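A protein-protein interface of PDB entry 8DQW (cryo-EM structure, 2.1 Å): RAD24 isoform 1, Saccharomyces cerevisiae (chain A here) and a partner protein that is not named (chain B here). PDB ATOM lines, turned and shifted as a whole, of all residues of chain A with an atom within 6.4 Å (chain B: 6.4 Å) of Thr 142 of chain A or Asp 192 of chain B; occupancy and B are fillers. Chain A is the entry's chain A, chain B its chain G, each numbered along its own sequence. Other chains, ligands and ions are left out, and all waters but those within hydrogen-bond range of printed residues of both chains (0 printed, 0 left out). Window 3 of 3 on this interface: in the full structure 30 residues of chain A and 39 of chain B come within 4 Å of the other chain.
The backbone carbonyl oxygen (O) of Thr 142 of chain A lies close to the side-chain amide oxygen (OD1) of Asn 144 of chain A, 3.1 Å away.
The backbone NH (N) of Phe 139 of chain A sits close to the side-chain amide nitrogen (ND2) of Asn 144 of chain A, 3.3 Å away.
O of Arg 140 of chain A is in hydrogen-bond range of OG of Ser 138 of chain A.
The guanidinium group of Arg 140 of chain A lies within salt-bridge range of the side-chain carboxylate of Asp 192 of chain B (3.8 Å).
Of the 7 printed residues of chain B, 4 touch a printed residue of chain A.
Among the printed residues, 5 pairs touch across the chains.
Thr 142 of chain A touches one residue of chain B.
Asp 192 of chain B touches two residues of chain A.
Of the printed residues of chain B, Arg 140 of chain A touches Trp 76, Asp 192 and Pro 193.
Printed residues of chain B within 4 Å of Phe 139 of chain A: Ile 194.
Of the printed residues of chain A, Pro 193 of chain B touches Arg 140 (3.7 Å).
Of the printed residues of chain A, Ile 194 of chain B touches Phe 139.
Of the printed residues of chain A, Trp 76 of chain B touches Arg 140.
Asn 144 of chain A touches none of the printed residues of chain B.
The nearest printed residue of chain B that does not touch Thr 142 of chain A is Pro 193 of chain B (6.9 Å).
The nearest residue of chain A that does not touch Asp 192 of chain B is Ser 141 of chain A (5.6 Å).
The nearest printed residue of chain B that does not touch Arg 140 of chain A is Ile 194 of chain B (4.1 Å).
Among the printed residues, merely in contact across the chains: Phe 139 of chain A with Ile 194 of chain B, Arg 140 of chain A with Trp 76 of chain B, Arg 140 of chain A with Pro 193 of chain B and Thr 142 of chain A with Asp 192 of chain B.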
ATOM      1  N   SER A 138       9.618 -17.900 -20.007  1.00  0.00           N
ATOM      2  CA  SER A 138       9.863 -18.765 -21.151  1.00  0.00           C
ATOM      3  C   SER A 138      11.364 -18.878 -21.351  1.00  0.00           C
ATOM      4  O   SER A 138      12.121 -17.983 -20.963  1.00  0.00           O
ATOM      5  CB  SER A 138       9.193 -18.227 -22.422  1.00  0.00           C
ATOM      6  OG  SER A 138       9.737 -16.972 -22.794  1.00  0.00           O
ATOM      7  N   PHE A 139      11.787 -19.988 -21.957  1.00  0.00           N
ATOM      8  CA  PHE A 139      13.209 -20.203 -22.198  1.00  0.00           C
ATOM      9  C   PHE A 139      13.798 -19.059 -23.015  1.00  0.00           C
ATOM     10  O   PHE A 139      14.646 -18.301 -22.533  1.00  0.00           O
ATOM     11  CB  PHE A 139      13.422 -21.542 -22.908  1.00  0.00           C
ATOM     12  CG  PHE A 139      13.587 -22.708 -21.971  1.00  0.00           C
ATOM     13  CD1 PHE A 139      12.780 -22.840 -20.853  1.00  0.00           C
ATOM     14  CD2 PHE A 139      14.551 -23.674 -22.212  1.00  0.00           C
ATOM     15  CE1 PHE A 139      12.930 -23.912 -19.992  1.00  0.00           C
ATOM     16  CE2 PHE A 139      14.706 -24.749 -21.353  1.00  0.00           C
ATOM     17  CZ  PHE A 139      13.895 -24.868 -20.244  1.00  0.00           C
ATOM     18  N   ARG A 140      13.338 -18.903 -24.252  1.00  0.00           N
ATOM     19  CA  ARG A 140      13.864 -17.913 -25.181  1.00  0.00           C
ATOM     20  C   ARG A 140      12.781 -16.889 -25.510  1.00  0.00           C
ATOM     21  O   ARG A 140      11.644 -16.975 -25.040  1.00  0.00           O
ATOM     22  CB  ARG A 140      14.386 -18.594 -26.451  1.00  0.00           C
ATOM     23  CG  ARG A 140      15.491 -19.607 -26.192  1.00  0.00           C
ATOM     24  CD  ARG A 140      15.747 -20.485 -27.407  1.00  0.00           C
ATOM     25  NE  ARG A 140      16.788 -21.475 -27.157  1.00  0.00           N
ATOM     26  CZ  ARG A 140      17.102 -22.463 -27.986  1.00  0.00           C
ATOM     27  NH1 ARG A 140      16.473 -22.625 -29.139  1.00  0.00           N
ATOM     28  NH2 ARG A 140      18.070 -23.309 -27.650  1.00  0.00           N
ATOM     29  N   SER A 141      13.152 -15.906 -26.334  1.00  0.00           N
ATOM     30  CA  SER A 141      12.206 -14.861 -26.711  1.00  0.00           C
ATOM     31  C   SER A 141      11.031 -15.438 -27.491  1.00  0.00           C
ATOM     32  O   SER A 141       9.889 -14.987 -27.335  1.00  0.00           O
ATOM     33  CB  SER A 141      12.916 -13.784 -27.531  1.00  0.00           C
ATOM     34  OG  SER A 141      12.068 -12.672 -27.755  1.00  0.00           O
ATOM     35  N   THR A 142      11.289 -16.434 -28.335  1.00  0.00           N
ATOM     36  CA  THR A 142      10.237 -17.037 -29.130  1.00  0.00           C
ATOM     37  C   THR A 142       9.252 -17.782 -28.231  1.00  0.00           C
ATOM     38  O   THR A 142       9.582 -18.149 -27.100  1.00  0.00           O
ATOM     39  CB  THR A 142      10.831 -17.997 -30.158  1.00  0.00           C
ATOM     40  OG1 THR A 142      11.804 -18.837 -29.526  1.00  0.00           O
ATOM     41  CG2 THR A 142      11.490 -17.223 -31.293  1.00  0.00           C
ATOM     42  N   PRO A 143       8.027 -18.017 -28.713  1.00  0.00           N
ATOM     43  CA  PRO A 143       7.030 -18.721 -27.891  1.00  0.00           C
ATOM     44  C   PRO A 143       7.341 -20.190 -27.651  1.00  0.00           C
ATOM     45  O   PRO A 143       6.505 -20.888 -27.065  1.00  0.00           O
ATOM     46  CB  PRO A 143       5.733 -18.558 -28.699  1.00  0.00           C
ATOM     47  CG  PRO A 143       6.176 -18.331 -30.098  1.00  0.00           C
ATOM     48  CD  PRO A 143       7.474 -17.588 -30.010  1.00  0.00           C
ATOM     49  N   ASN A 144       8.502 -20.687 -28.078  1.00  0.00           N
ATOM     50  CA  ASN A 144       8.902 -22.071 -27.840  1.00  0.00           C
ATOM     51  C   ASN A 144       7.883 -23.042 -28.441  1.00  0.00           C
ATOM     52  O   ASN A 144       7.232 -23.823 -27.744  1.00  0.00           O
ATOM     53  CB  ASN A 144       9.093 -22.328 -26.341  1.00  0.00           C
ATOM     54  CG  ASN A 144      10.090 -21.376 -25.711  1.00  0.00           C
ATOM     55  OD1 ASN A 144      10.948 -20.816 -26.391  1.00  0.00           O
ATOM     56  ND2 ASN A 144       9.978 -21.184 -24.401  1.00  0.00           N
ATOM     57  N   GLU A 145       7.755 -22.974 -29.766  1.00  0.00           N
ATOM     58  CA  GLU A 145       6.835 -23.836 -30.508  1.00  0.00           C
ATOM     59  C   GLU A 145       7.367 -25.267 -30.458  1.00  0.00           C
ATOM     60  O   GLU A 145       8.054 -25.749 -31.361  1.00  0.00           O
ATOM     61  CB  GLU A 145       6.682 -23.348 -31.944  1.00  0.00           C
ATOM     62  CG  GLU A 145       5.623 -24.092 -32.744  1.00  0.00           C
ATOM     63  CD  GLU A 145       5.618 -23.701 -34.209  1.00  0.00           C
ATOM     64  OE1 GLU A 145       6.420 -22.823 -34.594  1.00  0.00           O
ATOM     65  OE2 GLU A 145       4.815 -24.272 -34.976  1.00  0.00           O
ATOM     66  N   TRP B  76      27.069 -25.187 -24.472  1.00  0.00           N
ATOM     67  CA  TRP B  76      25.750 -25.357 -23.881  1.00  0.00           C
ATOM     68  C   TRP B  76      25.090 -26.624 -24.401  1.00  0.00           C
ATOM     69  O   TRP B  76      25.507 -27.221 -25.402  1.00  0.00           O
ATOM     70  CB  TRP B  76      24.855 -24.133 -24.135  1.00  0.00           C
ATOM     71  CG  TRP B  76      24.570 -23.838 -25.573  1.00  0.00           C
ATOM     72  CD1 TRP B  76      25.415 -23.265 -26.478  1.00  0.00           C
ATOM     73  CD2 TRP B  76      23.342 -24.083 -26.269  1.00  0.00           C
ATOM     74  NE1 TRP B  76      24.792 -23.145 -27.697  1.00  0.00           N
ATOM     75  CE2 TRP B  76      23.518 -23.639 -27.594  1.00  0.00           C
ATOM     76  CE3 TRP B  76      22.113 -24.637 -25.900  1.00  0.00           C
ATOM     77  CZ2 TRP B  76      22.512 -23.734 -28.553  1.00  0.00           C
ATOM     78  CZ3 TRP B  76      21.115 -24.731 -26.854  1.00  0.00           C
ATOM     79  CH2 TRP B  76      21.320 -24.281 -28.164  1.00  0.00           C
ATOM     80  N   GLN B 113      26.783 -15.871 -37.756  1.00  0.00           N
ATOM     81  CA  GLN B 113      25.625 -15.062 -37.411  1.00  0.00           C
ATOM     82  C   GLN B 113      26.065 -13.652 -37.046  1.00  0.00           C
ATOM     83  O   GLN B 113      27.169 -13.441 -36.536  1.00  0.00           O
ATOM     84  CB  GLN B 113      24.844 -15.658 -36.235  1.00  0.00           C
ATOM     85  CG  GLN B 113      23.658 -16.506 -36.634  1.00  0.00           C
ATOM     86  CD  GLN B 113      22.926 -17.066 -35.434  1.00  0.00           C
ATOM     87  OE1 GLN B 113      22.918 -18.273 -35.208  1.00  0.00           O
ATOM     88  NE2 GLN B 113      22.311 -16.187 -34.651  1.00  0.00           N
ATOM     89  N   LYS B 190      22.697 -22.456 -36.043  1.00  0.00           N
ATOM     90  CA  LYS B 190      22.345 -21.111 -35.621  1.00  0.00           C
ATOM     91  C   LYS B 190      22.188 -21.067 -34.106  1.00  0.00           C
ATOM     92  O   LYS B 190      21.838 -22.065 -33.471  1.00  0.00           O
ATOM     93  CB  LYS B 190      21.052 -20.645 -36.295  1.00  0.00           C
ATOM     94  CG  LYS B 190      21.155 -20.515 -37.806  1.00  0.00           C
ATOM     95  CD  LYS B 190      22.195 -19.482 -38.208  1.00  0.00           C
ATOM     96  CE  LYS B 190      21.853 -18.834 -39.537  1.00  0.00           C
ATOM     97  NZ  LYS B 190      23.069 -18.364 -40.255  1.00  0.00           N
ATOM     98  N   TYR B 191      22.457 -19.899 -33.533  1.00  0.00           N
ATOM     99  CA  TYR B 191      22.429 -19.696 -32.092  1.00  0.00           C
ATOM    100  C   TYR B 191      21.220 -18.852 -31.711  1.00  0.00           C
ATOM    101  O   TYR B 191      21.003 -17.778 -32.282  1.00  0.00           O
ATOM    102  CB  TYR B 191      23.714 -19.015 -31.615  1.00  0.00           C
ATOM    103  CG  TYR B 191      23.771 -18.795 -30.122  1.00  0.00           C
ATOM    104  CD1 TYR B 191      23.571 -19.845 -29.238  1.00  0.00           C
ATOM    105  CD2 TYR B 191      24.029 -17.536 -29.596  1.00  0.00           C
ATOM    106  CE1 TYR B 191      23.624 -19.649 -27.872  1.00  0.00           C
ATOM    107  CE2 TYR B 191      24.085 -17.331 -28.233  1.00  0.00           C
ATOM    108  CZ  TYR B 191      23.882 -18.390 -27.375  1.00  0.00           C
ATOM    109  OH  TYR B 191      23.935 -18.191 -26.015  1.00  0.00           O
ATOM    110  N   ASP B 192      20.447 -19.339 -30.744  1.00  0.00           N
ATOM    111  CA  ASP B 192      19.282 -18.625 -30.221  1.00  0.00           C
ATOM    112  C   ASP B 192      19.504 -18.356 -28.738  1.00  0.00           C
ATOM    113  O   ASP B 192      19.263 -19.245 -27.903  1.00  0.00           O
ATOM    114  CB  ASP B 192      18.005 -19.434 -30.438  1.00  0.00           C
ATOM    115  CG  ASP B 192      16.755 -18.575 -30.397  1.00  0.00           C
ATOM    116  OD1 ASP B 192      16.882 -17.340 -30.275  1.00  0.00           O
ATOM    117  OD2 ASP B 192      15.643 -19.138 -30.487  1.00  0.00           O
ATOM    118  N   PRO B 193      19.968 -17.165 -28.357  1.00  0.00           N
ATOM    119  CA  PRO B 193      20.275 -16.920 -26.942  1.00  0.00           C
ATOM    120  C   PRO B 193      19.058 -17.112 -26.050  1.00  0.00           C
ATOM    121  O   PRO B 193      17.922 -16.824 -26.433  1.00  0.00           O
ATOM    122  CB  PRO B 193      20.753 -15.459 -26.921  1.00  0.00           C
ATOM    123  CG  PRO B 193      20.514 -14.917 -28.296  1.00  0.00           C
ATOM    124  CD  PRO B 193      20.456 -16.077 -29.219  1.00  0.00           C
ATOM    125  N   ILE B 194      19.313 -17.613 -24.844  1.00  0.00           N
ATOM    126  CA  ILE B 194      18.291 -17.781 -23.818  1.00  0.00           C
ATOM    127  C   ILE B 194      18.337 -16.562 -22.907  1.00  0.00           C
ATOM    128  O   ILE B 194      19.414 -16.155 -22.454  1.00  0.00           O
ATOM    129  CB  ILE B 194      18.505 -19.086 -23.028  1.00  0.00           C
ATOM    130  CG1 ILE B 194      17.174 -19.602 -22.476  1.00  0.00           C
ATOM    131  CG2 ILE B 194      19.512 -18.893 -21.900  1.00  0.00           C
ATOM    132  CD1 ILE B 194      17.251 -20.998 -21.895  1.00  0.00           C
